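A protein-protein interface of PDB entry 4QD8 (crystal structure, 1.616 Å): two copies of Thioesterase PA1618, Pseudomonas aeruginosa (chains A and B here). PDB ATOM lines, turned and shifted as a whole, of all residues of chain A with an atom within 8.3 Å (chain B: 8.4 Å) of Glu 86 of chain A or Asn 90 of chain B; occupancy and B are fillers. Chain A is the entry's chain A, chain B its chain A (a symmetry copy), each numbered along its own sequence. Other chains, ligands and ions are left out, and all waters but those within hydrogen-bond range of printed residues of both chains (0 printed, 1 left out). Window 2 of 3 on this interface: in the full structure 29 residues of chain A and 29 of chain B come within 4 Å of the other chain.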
ATOM      1  N   VAL A  60     -15.581  26.318 -15.058  1.00  0.00           N
ATOM      2  CA  VAL A  60     -15.016  26.498 -13.726  1.00  0.00           C
ATOM      3  C   VAL A  60     -15.592  27.756 -13.042  1.00  0.00           C
ATOM      4  O   VAL A  60     -15.860  27.728 -11.841  1.00  0.00           O
ATOM      5  CB  VAL A  60     -13.473  26.456 -13.736  1.00  0.00           C
ATOM      6  CG1 VAL A  60     -12.914  26.685 -12.315  1.00  0.00           C
ATOM      7  CG2 VAL A  60     -12.991  25.098 -14.262  1.00  0.00           C
ATOM      8  N   GLU A  64     -17.253  27.445  -9.481  1.00  0.00           N
ATOM      9  CA  GLU A  64     -16.739  28.219  -8.345  1.00  0.00           C
ATOM     10  C   GLU A  64     -17.772  29.227  -7.832  1.00  0.00           C
ATOM     11  O   GLU A  64     -17.848  29.467  -6.624  1.00  0.00           O
ATOM     12  CB  GLU A  64     -15.382  28.876  -8.662  1.00  0.00           C
ATOM     13  CG  GLU A  64     -14.721  29.451  -7.418  1.00  0.00           C
ATOM     14  CD  GLU A  64     -13.190  29.429  -7.429  1.00  0.00           C
ATOM     15  OE1 GLU A  64     -12.550  28.637  -8.180  1.00  0.00           O
ATOM     16  OE2 GLU A  64     -12.643  30.209  -6.635  1.00  0.00           O
ATOM     17  N   VAL A  83     -13.367  32.036   0.798  1.00  0.00           N
ATOM     18  CA  VAL A  83     -12.718  32.279  -0.491  1.00  0.00           C
ATOM     19  C   VAL A  83     -12.249  30.960  -1.099  1.00  0.00           C
ATOM     20  O   VAL A  83     -11.949  30.007  -0.383  1.00  0.00           O
ATOM     21  CB  VAL A  83     -11.532  33.244  -0.356  1.00  0.00           C
ATOM     22  CG1 VAL A  83     -12.010  34.603   0.154  1.00  0.00           C
ATOM     23  CG2 VAL A  83     -10.479  32.683   0.580  1.00  0.00           C
ATOM     24  N   GLY A  84     -12.199  30.895  -2.423  1.00  0.00           N
ATOM     25  CA  GLY A  84     -11.671  29.708  -3.076  1.00  0.00           C
ATOM     26  C   GLY A  84     -10.229  29.459  -2.680  1.00  0.00           C
ATOM     27  O   GLY A  84      -9.407  30.380  -2.663  1.00  0.00           O
ATOM     28  N   LEU A  85      -9.899  28.202  -2.392  1.00  0.00           N
ATOM     29  CA  LEU A  85      -8.533  27.837  -2.050  1.00  0.00           C
ATOM     30  C   LEU A  85      -7.904  26.944  -3.120  1.00  0.00           C
ATOM     31  O   LEU A  85      -6.774  27.169  -3.539  1.00  0.00           O
ATOM     32  CB  LEU A  85      -8.497  27.150  -0.681  1.00  0.00           C
ATOM     33  CG  LEU A  85      -7.134  26.746  -0.120  1.00  0.00           C
ATOM     34  CD1 LEU A  85      -6.343  27.990   0.230  1.00  0.00           C
ATOM     35  CD2 LEU A  85      -7.296  25.847   1.106  1.00  0.00           C
ATOM     36  N   GLU A  86      -8.634  25.920  -3.540  1.00  0.00           N
ATOM     37  CA  GLU A  86      -8.148  25.037  -4.598  1.00  0.00           C
ATOM     38  C   GLU A  86      -9.322  24.602  -5.440  1.00  0.00           C
ATOM     39  O   GLU A  86     -10.405  24.355  -4.926  1.00  0.00           O
ATOM     40  CB  GLU A  86      -7.461  23.804  -3.993  1.00  0.00           C
ATOM     41  CG  GLU A  86      -6.328  23.227  -4.867  1.00  0.00           C
ATOM     42  CD  GLU A  86      -6.810  22.260  -5.915  1.00  0.00           C
ATOM     43  OE1 GLU A  86      -7.975  21.812  -5.842  1.00  0.00           O
ATOM     44  OE2 GLU A  86      -5.998  21.933  -6.815  1.00  0.00           O
ATOM     45  N   VAL A  87      -9.126  24.502  -6.746  1.00  0.00           N
ATOM     46  CA  VAL A  87     -10.203  24.012  -7.594  1.00  0.00           C
ATOM     47  C   VAL A  87      -9.604  23.097  -8.642  1.00  0.00           C
ATOM     48  O   VAL A  87      -8.473  23.290  -9.073  1.00  0.00           O
ATOM     49  CB  VAL A  87     -11.002  25.175  -8.256  1.00  0.00           C
ATOM     50  CG1 VAL A  87     -10.144  25.970  -9.258  1.00  0.00           C
ATOM     51  CG2 VAL A  87     -12.281  24.641  -8.907  1.00  0.00           C
ATOM     52  N   ASN A  88     -10.364  22.093  -9.042  1.00  0.00           N
ATOM     53  CA  ASN A  88      -9.924  21.214 -10.118  1.00  0.00           C
ATOM     54  C   ASN A  88     -11.145  20.747 -10.887  1.00  0.00           C
ATOM     55  O   ASN A  88     -12.256  20.780 -10.373  1.00  0.00           O
ATOM     56  CB  ASN A  88      -9.109  20.032  -9.585  1.00  0.00           C
ATOM     57  CG  ASN A  88      -9.876  19.190  -8.570  1.00  0.00           C
ATOM     58  OD1 ASN A  88     -10.817  18.474  -8.916  1.00  0.00           O
ATOM     59  ND2 ASN A  88      -9.497  19.308  -7.301  1.00  0.00           N
ATOM     60  N   ALA A  89     -10.951  20.354 -12.136  1.00  0.00           N
ATOM     61  CA  ALA A  89     -12.078  19.898 -12.945  1.00  0.00           C
ATOM     62  C   ALA A  89     -11.604  18.956 -14.036  1.00  0.00           C
ATOM     63  O   ALA A  89     -10.525  19.141 -14.595  1.00  0.00           O
ATOM     64  CB  ALA A  89     -12.796  21.095 -13.569  1.00  0.00           C
ATOM     65  N   THR A 113     -12.006  24.599   6.272  1.00  0.00           N
ATOM     66  CA  THR A 113     -12.149  24.346   4.832  1.00  0.00           C
ATOM     67  C   THR A 113     -13.472  23.679   4.520  1.00  0.00           C
ATOM     68  O   THR A 113     -14.026  22.964   5.350  1.00  0.00           O
ATOM     69  CB  THR A 113     -11.031  23.434   4.275  1.00  0.00           C
ATOM     70  OG1 THR A 113     -11.088  22.167   4.939  1.00  0.00           O
ATOM     71  CG2 THR A 113      -9.658  24.063   4.457  1.00  0.00           C
ATOM     72  N   HIS A 114     -13.977  23.917   3.312  1.00  0.00           N
ATOM     73  CA  HIS A 114     -15.159  23.225   2.818  1.00  0.00           C
ATOM     74  C   HIS A 114     -14.751  22.570   1.523  1.00  0.00           C
ATOM     75  O   HIS A 114     -13.963  23.139   0.769  1.00  0.00           O
ATOM     76  CB  HIS A 114     -16.282  24.204   2.476  1.00  0.00           C
ATOM     77  CG  HIS A 114     -16.924  24.854   3.657  1.00  0.00           C
ATOM     78  ND1 HIS A 114     -17.864  25.856   3.525  1.00  0.00           N
ATOM     79  CD2 HIS A 114     -16.766  24.657   4.991  1.00  0.00           C
ATOM     80  CE1 HIS A 114     -18.268  26.236   4.727  1.00  0.00           C
ATOM     81  NE2 HIS A 114     -17.612  25.536   5.631  1.00  0.00           N
ATOM     82  N   VAL A 115     -15.296  21.393   1.257  1.00  0.00           N
ATOM     83  CA  VAL A 115     -15.051  20.719  -0.023  1.00  0.00           C
ATOM     84  C   VAL A 115     -16.404  20.420  -0.672  1.00  0.00           C
ATOM     85  O   VAL A 115     -17.277  19.792  -0.059  1.00  0.00           O
ATOM     86  CB  VAL A 115     -14.227  19.428   0.168  1.00  0.00           C
ATOM     87  CG1 VAL A 115     -13.930  18.770  -1.189  1.00  0.00           C
ATOM     88  CG2 VAL A 115     -12.913  19.714   0.891  1.00  0.00           C
ATOM     89  N   TRP A 116     -16.572  20.873  -1.918  1.00  0.00           N
ATOM     90  CA  TRP A 116     -17.810  20.713  -2.683  1.00  0.00           C
ATOM     91  C   TRP A 116     -17.582  19.840  -3.919  1.00  0.00           C
ATOM     92  O   TRP A 116     -16.545  19.966  -4.579  1.00  0.00           O
ATOM     93  CB  TRP A 116     -18.320  22.086  -3.151  1.00  0.00           C
ATOM     94  CG  TRP A 116     -18.750  22.965  -2.015  1.00  0.00           C
ATOM     95  CD1 TRP A 116     -18.027  23.963  -1.430  1.00  0.00           C
ATOM     96  CD2 TRP A 116     -19.989  22.891  -1.306  1.00  0.00           C
ATOM     97  NE1 TRP A 116     -18.753  24.522  -0.394  1.00  0.00           N
ATOM     98  CE2 TRP A 116     -19.962  23.880  -0.301  1.00  0.00           C
ATOM     99  CE3 TRP A 116     -21.121  22.075  -1.417  1.00  0.00           C
ATOM    100  CZ2 TRP A 116     -21.032  24.082   0.593  1.00  0.00           C
ATOM    101  CZ3 TRP A 116     -22.194  22.285  -0.531  1.00  0.00           C
ATOM    102  CH2 TRP A 116     -22.129  23.279   0.457  1.00  0.00           C
ATOM    103  N   ALA A 131     -16.261  18.914 -11.202  1.00  0.00           N
ATOM    104  CA  ALA A 131     -15.317  19.791 -10.523  1.00  0.00           C
ATOM    105  C   ALA A 131     -15.283  19.460  -9.048  1.00  0.00           C
ATOM    106  O   ALA A 131     -16.265  18.969  -8.497  1.00  0.00           O
ATOM    107  CB  ALA A 131     -15.687  21.259 -10.725  1.00  0.00           C
ATOM    108  N   ARG A 132     -14.148  19.722  -8.414  1.00  0.00           N
ATOM    109  CA  ARG A 132     -14.105  19.689  -6.954  1.00  0.00           C
ATOM    110  C   ARG A 132     -13.498  20.982  -6.445  1.00  0.00           C
ATOM    111  O   ARG A 132     -12.474  21.472  -6.949  1.00  0.00           O
ATOM    112  CB  ARG A 132     -13.373  18.450  -6.423  1.00  0.00           C
ATOM    113  CG  ARG A 132     -13.629  18.224  -4.916  1.00  0.00           C
ATOM    114  CD  ARG A 132     -13.124  16.864  -4.427  1.00  0.00           C
ATOM    115  NE  ARG A 132     -11.673  16.825  -4.385  1.00  0.00           N
ATOM    116  CZ  ARG A 132     -10.902  16.220  -5.281  1.00  0.00           C
ATOM    117  NH1 ARG A 132     -11.444  15.542  -6.288  1.00  0.00           N
ATOM    118  NH2 ARG A 132      -9.586  16.281  -5.155  1.00  0.00           N
ATOM    119  N   LEU A 133     -14.166  21.579  -5.466  1.00  0.00           N
ATOM    120  CA  LEU A 133     -13.768  22.895  -4.988  1.00  0.00           C
ATOM    121  C   LEU A 133     -13.471  22.857  -3.496  1.00  0.00           C
ATOM    122  O   LEU A 133     -14.270  22.336  -2.719  1.00  0.00           O
ATOM    123  CB  LEU A 133     -14.910  23.889  -5.223  1.00  0.00           C
ATOM    124  CG  LEU A 133     -14.695  25.321  -4.707  1.00  0.00           C
ATOM    125  CD1 LEU A 133     -13.521  26.002  -5.396  1.00  0.00           C
ATOM    126  CD2 LEU A 133     -16.005  26.116  -4.933  1.00  0.00           C
ATOM    127  N   THR A 134     -12.309  23.378  -3.122  1.00  0.00           N
ATOM    128  CA  THR A 134     -11.948  23.590  -1.710  1.00  0.00           C
ATOM    129  C   THR A 134     -12.012  25.080  -1.378  1.00  0.00           C
ATOM    130  O   THR A 134     -11.305  25.885  -1.980  1.00  0.00           O
ATOM    131  CB  THR A 134     -10.545  23.078  -1.436  1.00  0.00           C
ATOM    132  OG1 THR A 134     -10.471  21.711  -1.853  1.00  0.00           O
ATOM    133  CG2 THR A 134     -10.192  23.177   0.073  1.00  0.00           C
ATOM    134  N   MET A 135     -12.869  25.434  -0.416  1.00  0.00           N
ATOM    135  CA  MET A 135     -13.013  26.813   0.049  1.00  0.00           C
ATOM    136  C   MET A 135     -12.282  26.960   1.369  1.00  0.00           C
ATOM    137  O   MET A 135     -12.260  26.033   2.168  1.00  0.00           O
ATOM    138  CB  MET A 135     -14.496  27.131   0.287  1.00  0.00           C
ATOM    139  CG  MET A 135     -15.369  27.035  -0.958  1.00  0.00           C
ATOM    140  SD  MET A 135     -14.954  28.291  -2.180  1.00  0.00           S
ATOM    141  CE  MET A 135     -15.370  29.799  -1.290  1.00  0.00           C
ATOM    142  N   ALA A 136     -11.675  28.122   1.590  1.00  0.00           N
ATOM    143  CA  ALA A 136     -11.121  28.455   2.903  1.00  0.00           C
ATOM    144  C   ALA A 136     -12.163  29.253   3.681  1.00  0.00           C
ATOM    145  O   ALA A 136     -12.836  30.120   3.133  1.00  0.00           O
ATOM    146  CB  ALA A 136      -9.859  29.255   2.761  1.00  0.00           C
ATOM    147  N   GLY B  56     -12.207  33.367  -8.596  1.00  0.00           N
ATOM    148  CA  GLY B  56     -11.222  32.320  -8.811  1.00  0.00           C
ATOM    149  C   GLY B  56     -11.431  31.612 -10.133  1.00  0.00           C
ATOM    150  O   GLY B  56     -10.479  31.162 -10.769  1.00  0.00           O
ATOM    151  N   SER B  59      -9.669  33.558 -12.883  1.00  0.00           N
ATOM    152  CA  SER B  59      -8.256  33.195 -12.957  1.00  0.00           C
ATOM    153  C   SER B  59      -8.092  31.957 -13.819  1.00  0.00           C
ATOM    154  O   SER B  59      -7.146  31.867 -14.610  1.00  0.00           O
ATOM    155  CB  SER B  59      -7.659  32.922 -11.577  1.00  0.00           C
ATOM    156  OG  SER B  59      -7.417  34.135 -10.889  1.00  0.00           O
ATOM    157  N   VAL B  60      -9.021  31.018 -13.680  1.00  0.00           N
ATOM    158  CA  VAL B  60      -8.948  29.782 -14.451  1.00  0.00           C
ATOM    159  C   VAL B  60      -9.284  30.032 -15.936  1.00  0.00           C
ATOM    160  O   VAL B  60      -8.646  29.449 -16.812  1.00  0.00           O
ATOM    161  CB  VAL B  60      -9.779  28.648 -13.815  1.00  0.00           C
ATOM    162  CG1 VAL B  60      -9.704  27.370 -14.678  1.00  0.00           C
ATOM    163  CG2 VAL B  60      -9.256  28.344 -12.405  1.00  0.00           C
ATOM    164  N   GLU B  86      -8.099  18.406 -18.280  1.00  0.00           N
ATOM    165  CA  GLU B  86      -8.135  18.544 -16.825  1.00  0.00           C
ATOM    166  C   GLU B  86      -7.491  19.855 -16.450  1.00  0.00           C
ATOM    167  O   GLU B  86      -6.506  20.266 -17.050  1.00  0.00           O
ATOM    168  CB  GLU B  86      -7.376  17.386 -16.159  1.00  0.00           C
ATOM    169  CG  GLU B  86      -7.924  16.995 -14.770  1.00  0.00           C
ATOM    170  CD  GLU B  86      -7.355  17.819 -13.646  1.00  0.00           C
ATOM    171  OE1 GLU B  86      -6.350  18.532 -13.860  1.00  0.00           O
ATOM    172  OE2 GLU B  86      -7.917  17.735 -12.528  1.00  0.00           O
ATOM    173  N   VAL B  87      -8.036  20.533 -15.451  1.00  0.00           N
ATOM    174  CA  VAL B  87      -7.408  21.765 -14.997  1.00  0.00           C
ATOM    175  C   VAL B  87      -7.479  21.808 -13.485  1.00  0.00           C
ATOM    176  O   VAL B  87      -8.418  21.297 -12.885  1.00  0.00           O
ATOM    177  CB  VAL B  87      -8.075  23.027 -15.625  1.00  0.00           C
ATOM    178  CG1 VAL B  87      -9.527  23.213 -15.145  1.00  0.00           C
ATOM    179  CG2 VAL B  87      -7.226  24.272 -15.351  1.00  0.00           C
ATOM    180  N   ASN B  88      -6.476  22.409 -12.871  1.00  0.00           N
ATOM    181  CA  ASN B  88      -6.495  22.592 -11.426  1.00  0.00           C
ATOM    182  C   ASN B  88      -5.774  23.885 -11.095  1.00  0.00           C
ATOM    183  O   ASN B  88      -4.979  24.375 -11.888  1.00  0.00           O
ATOM    184  CB  ASN B  88      -5.874  21.398 -10.696  1.00  0.00           C
ATOM    185  CG  ASN B  88      -4.433  21.127 -11.118  1.00  0.00           C
ATOM    186  OD1 ASN B  88      -3.519  21.888 -10.796  1.00  0.00           O
ATOM    187  ND2 ASN B  88      -4.235  20.056 -11.880  1.00  0.00           N
ATOM    188  N   ALA B  89      -6.080  24.465  -9.945  1.00  0.00           N
ATOM    189  CA  ALA B  89      -5.435  25.717  -9.560  1.00  0.00           C
ATOM    190  C   ALA B  89      -5.433  25.872  -8.050  1.00  0.00           C
ATOM    191  O   ALA B  89      -6.387  25.480  -7.381  1.00  0.00           O
ATOM    192  CB  ALA B  89      -6.157  26.901 -10.202  1.00  0.00           C
ATOM    193  N   ASN B  90      -4.347  26.424  -7.527  1.00  0.00           N
ATOM    194  CA  ASN B  90      -4.372  26.962  -6.156  1.00  0.00           C
ATOM    195  C   ASN B  90      -4.534  28.471  -6.200  1.00  0.00           C
ATOM    196  O   ASN B  90      -3.786  29.161  -6.886  1.00  0.00           O
ATOM    197  CB  ASN B  90      -3.086  26.611  -5.404  1.00  0.00           C
ATOM    198  CG  ASN B  90      -3.174  25.285  -4.688  1.00  0.00           C
ATOM    199  OD1 ASN B  90      -3.450  25.222  -3.477  1.00  0.00           O
ATOM    200  ND2 ASN B  90      -2.947  24.211  -5.420  1.00  0.00           N
ATOM    201  N   HIS B  91      -5.513  28.982  -5.452  1.00  0.00           N
ATOM    202  CA  HIS B  91      -5.706  30.406  -5.269  1.00  0.00           C
ATOM    203  C   HIS B  91      -4.873  30.856  -4.063  1.00  0.00           C
ATOM    204  O   HIS B  91      -5.137  30.466  -2.925  1.00  0.00           O
ATOM    205  CB  HIS B  91      -7.207  30.706  -5.083  1.00  0.00           C
ATOM    206  CG  HIS B  91      -8.065  30.187  -6.197  1.00  0.00           C
ATOM    207  ND1 HIS B  91      -7.871  30.546  -7.520  1.00  0.00           N
ATOM    208  CD2 HIS B  91      -9.126  29.347  -6.191  1.00  0.00           C
ATOM    209  CE1 HIS B  91      -8.770  29.944  -8.271  1.00  0.00           C
ATOM    210  NE2 HIS B  91      -9.545  29.205  -7.497  1.00  0.00           N
ATOM    211  N   LEU B  92      -3.835  31.636  -4.341  1.00  0.00           N
ATOM    212  CA  LEU B  92      -2.809  31.989  -3.366  1.00  0.00           C
ATOM    213  C   LEU B  92      -3.070  33.314  -2.650  1.00  0.00           C
ATOM    214  O   LEU B  92      -2.917  33.411  -1.432  1.00  0.00           O
ATOM    215  CB  LEU B  92      -1.453  32.084  -4.052  1.00  0.00           C
ATOM    216  CG  LEU B  92      -1.067  30.868  -4.893  1.00  0.00           C
ATOM    217  CD1 LEU B  92       0.233  31.148  -5.617  1.00  0.00           C
ATOM    218  CD2 LEU B  92      -0.953  29.621  -4.003  1.00  0.00           C
ATOM    219  N   ARG B  93      -3.416  34.338  -3.423  1.00  0.00           N
ATOM    220  CA  ARG B  93      -3.657  35.685  -2.895  1.00  0.00           C
ATOM    221  C   ARG B  93      -4.845  36.301  -3.598  1.00  0.00           C
ATOM    222  O   ARG B  93      -5.014  36.143  -4.808  1.00  0.00           O
ATOM    223  CB  ARG B  93      -2.440  36.583  -3.134  1.00  0.00           C
ATOM    224  CG  ARG B  93      -1.256  36.292  -2.216  1.00  0.00           C
ATOM    225  CD  ARG B  93      -0.121  37.265  -2.453  1.00  0.00           C
ATOM    226  NE  ARG B  93       0.974  37.067  -1.505  1.00  0.00           N
ATOM    227  CZ  ARG B  93       1.932  36.158  -1.660  1.00  0.00           C
ATOM    228  NH1 ARG B  93       1.924  35.362  -2.723  1.00  0.00           N
ATOM    229  NH2 ARG B  93       2.898  36.040  -0.752  1.00  0.00           N
ATOM    230  N   ILE B 118       1.041  27.204 -15.347  1.00  0.00           N
ATOM    231  CA  ILE B 118       0.610  28.588 -15.548  1.00  0.00           C
ATOM    232  C   ILE B 118       0.682  29.356 -14.233  1.00  0.00           C
ATOM    233  O   ILE B 118       0.064  28.962 -13.242  1.00  0.00           O
ATOM    234  CB  ILE B 118      -0.792  28.655 -16.182  1.00  0.00           C
ATOM    235  CG1 ILE B 118      -0.754  27.933 -17.533  1.00  0.00           C
ATOM    236  CG2 ILE B 118      -1.214  30.112 -16.413  1.00  0.00           C
ATOM    237  CD1 ILE B 118      -2.044  27.282 -17.914  1.00  0.00           C
ATOM    238  N   LEU B 120       0.248  32.993 -12.155  1.00  0.00           N
ATOM    239  CA  LEU B 120      -0.456  34.273 -12.196  1.00  0.00           C
ATOM    240  C   LEU B 120       0.010  35.169 -11.063  1.00  0.00           C
ATOM    241  O   LEU B 120       0.333  34.692  -9.963  1.00  0.00           O
ATOM    242  CB  LEU B 120      -1.976  34.081 -12.085  1.00  0.00           C
ATOM    243  CG  LEU B 120      -2.728  33.620 -13.335  1.00  0.00           C
ATOM    244  CD1 LEU B 120      -2.372  32.184 -13.668  1.00  0.00           C
ATOM    245  CD2 LEU B 120      -4.219  33.753 -13.137  1.00  0.00           C
ATOM    246  N   PRO B 127       2.849  36.156  -6.330  1.00  0.00           N
ATOM    247  CA  PRO B 127       2.028  35.051  -6.852  1.00  0.00           C
ATOM    248  C   PRO B 127       0.598  35.094  -6.314  1.00  0.00           C
ATOM    249  O   PRO B 127       0.397  35.155  -5.085  1.00  0.00           O
ATOM    250  CB  PRO B 127       2.744  33.809  -6.319  1.00  0.00           C
ATOM    251  CG  PRO B 127       4.193  34.219  -6.254  1.00  0.00           C
ATOM    252  CD  PRO B 127       4.155  35.688  -5.829  1.00  0.00           C
ATOM    253  N   SER B 128      -0.380  35.047  -7.219  1.00  0.00           N
ATOM    254  CA  SER B 128      -1.785  35.114  -6.833  1.00  0.00           C
ATOM    255  C   SER B 128      -2.520  33.807  -7.112  1.00  0.00           C
ATOM    256  O   SER B 128      -3.524  33.505  -6.483  1.00  0.00           O
ATOM    257  CB  SER B 128      -2.500  36.265  -7.545  1.00  0.00           C
ATOM    258  OG  SER B 128      -2.467  36.110  -8.961  1.00  0.00           O
ATOM    259  N   CYS B 129      -2.026  33.046  -8.087  1.00  0.00           N
ATOM    260  CA  CYS B 129      -2.654  31.770  -8.430  1.00  0.00           C
ATOM    261  C   CYS B 129      -1.626  30.934  -9.189  1.00  0.00           C
ATOM    262  O   CYS B 129      -0.794  31.474  -9.923  1.00  0.00           O
ATOM    263  CB  CYS B 129      -3.911  32.019  -9.284  1.00  0.00           C
ATOM    264  SG  CYS B 129      -4.768  30.554  -9.906  1.00  0.00           S
ATOM    265  N   ILE B 130      -1.657  29.619  -8.982  1.00  0.00           N
ATOM    266  CA  ILE B 130      -0.860  28.735  -9.820  1.00  0.00           C
ATOM    267  C   ILE B 130      -1.804  27.700 -10.398  1.00  0.00           C
ATOM    268  O   ILE B 130      -2.631  27.145  -9.678  1.00  0.00           O
ATOM    269  CB  ILE B 130       0.320  28.065  -9.067  1.00  0.00           C
ATOM    270  CG1 ILE B 130       1.031  27.062  -9.989  1.00  0.00           C
ATOM    271  CG2 ILE B 130      -0.144  27.373  -7.761  1.00  0.00           C
ATOM    272  CD1 ILE B 130       2.353  26.564  -9.411  1.00  0.00           C
ATOM    273  N   ALA B 131      -1.706  27.451 -11.702  1.00  0.00           N
ATOM    274  CA  ALA B 131      -2.610  26.507 -12.345  1.00  0.00           C
ATOM    275  C   ALA B 131      -1.810  25.460 -13.088  1.00  0.00           C
ATOM    276  O   ALA B 131      -0.688  25.721 -13.516  1.00  0.00           O
ATOM    277  CB  ALA B 131      -3.560  27.222 -13.304  1.00  0.00           C
ATOM    278  N   ARG B 132      -2.386  24.274 -13.230  1.00  0.00           N
ATOM    279  CA  ARG B 132      -1.816  23.295 -14.152  1.00  0.00           C
ATOM    280  C   ARG B 132      -2.904  22.796 -15.084  1.00  0.00           C
ATOM    281  O   ARG B 132      -4.030  22.474 -14.669  1.00  0.00           O
ATOM    282  CB  ARG B 132      -1.107  22.150 -13.416  1.00  0.00           C
ATOM    283  CG  ARG B 132      -0.211  21.318 -14.359  1.00  0.00           C
ATOM    284  CD  ARG B 132       0.697  20.342 -13.607  1.00  0.00           C
ATOM    285  NE  ARG B 132      -0.065  19.241 -13.043  1.00  0.00           N
ATOM    286  CZ  ARG B 132      -0.400  19.125 -11.763  1.00  0.00           C
ATOM    287  NH1 ARG B 132       0.007  20.028 -10.876  1.00  0.00           N
ATOM    288  NH2 ARG B 132      -1.127  18.091 -11.372  1.00  0.00           N
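Val 60 of chain A touches its own counterpart, Val 60 of chain B. Glu 86 of chain A touches Asn 88 of chain B, and with the chains exchanged Asn 88 of chain A touches Glu 86 of chain B. Val 87 of chain A touches Ala 89 of chain B, and with the chains exchanged Ala 89 of chain A touches Val 87 of chain B. Asn 88 of chain B touches its own counterpart, Asn 88 of chain A.
Among the printed residues, merely in contact across the chains: Asn 88 of chain A with Val 87 of chain B, Val 87 of chain A with Asn 88 of chain B, Gly 84 of chain A with His 91 of chain B, Ala 89 of chain A with Glu 86 of chain B, Glu 86 of chain A with Ala 89 of chain B, Glu 64 of chain A with Gly 56 of chain B, Leu 85 of chain A with Asn 90 of chain B, Glu 86 of chain A with Asn 90 of chain B, Asn 88 of chain A with Asn 88 of chain B, Val 87 of chain A with His 91 of chain B, Asn 88 of chain A with Glu 86 of chain B, Glu 86 of chain A with Asn 88 of chain B and Val 60 of chain A with Val 60 of chain B.
Hydrophobic or aromatic side chains of chain B that line the printed part of chain A: Val 60 and His 91. Hydrophobic or aromatic side chains of chain A within 4 Å of the printed part of chain B: Val 60 and Val 87. Among the printed residues, 17 pairs touch across the chains. Among the printed residues, no Asp or Glu carboxylate lies within 4 Å of a Lys or Arg side-chain nitrogen of the other chain.
Of chain B, only Asn 88 (3.9 Å), Ala 89 (3.3 Å) and Asn 90 (3.6 Å) come within 4 Å of Glu 86 of chain A. Printed residues of chain A within 4 Å of Ala 89 of chain B: Glu 86 (3.3 Å) and Val 87 (2.8 Å). Of the printed residues of chain A, Asn 88 of chain B touches Glu 86 (3.9 Å), Val 87 (3.2 Å) and Asn 88 (3.7 Å). Printed residues of chain B within 4 Å of Leu 85 of chain A: Asn 90 and His 91. Printed residues of chain B within 4 Å of Asn 88 of chain A: Glu 86, Val 87 and Asn 88. Of the printed residues of chain B, Ala 89 of chain A touches Glu 86 and Val 87. Leu 133 of chain A touches none of the printed residues of chain B. Thr 134 of chain A touches none of the printed residues of chain B. The nearest residue of chain B that does not touch Glu 86 of chain A is His 91 of chain B (4.4 Å). The nearest residue of chain A that does not touch Asn 90 of chain B is Val 87 of chain A (5.2 Å).
N of Gly 84 of chain A lies close to SD of Met 135 of chain A (3.8 Å). The backbone NH of Leu 85 of chain A is in hydrogen-bond range of the backbone carbonyl oxygen of Thr 134 of chain A. The backbone NH (N) of Arg 132 of chain A lies within hydrogen-bond range of the backbone carbonyl oxygen (O) of Asn 88 of chain A (2.9 Å). OE1 of Glu 86 of chain B sits at hydrogen-bond distance from ND2 of Asn 88 of chain B (3.3 Å). The backbone carbonyl oxygen (O) of Asn 90 of chain B lies close to the side-chain sulfur (SG) of Cys 129 of chain B. The backbone carbonyl oxygen (O) of Ile 130 of chain B sits at hydrogen-bond distance from the backbone NH (N) of Asn 90 of chain B, at 2.8 Å.
The side-chain carboxylate of Glu 64 of chain A sits at hydrogen-bond distance from a ring nitrogen (NE2) of His 91 of chain B, at 3.1 Å. O of Leu 85 of chain A sits at hydrogen-bond distance from N of His 91 of chain B. O of Val 87 of chain A is in hydrogen-bond range of N of Ala 89 of chain B (2.8 Å). The backbone carbonyl oxygen (O) of Val 87 of chain B sits at hydrogen-bond distance from the backbone NH (N) of Ala 89 of chain A.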
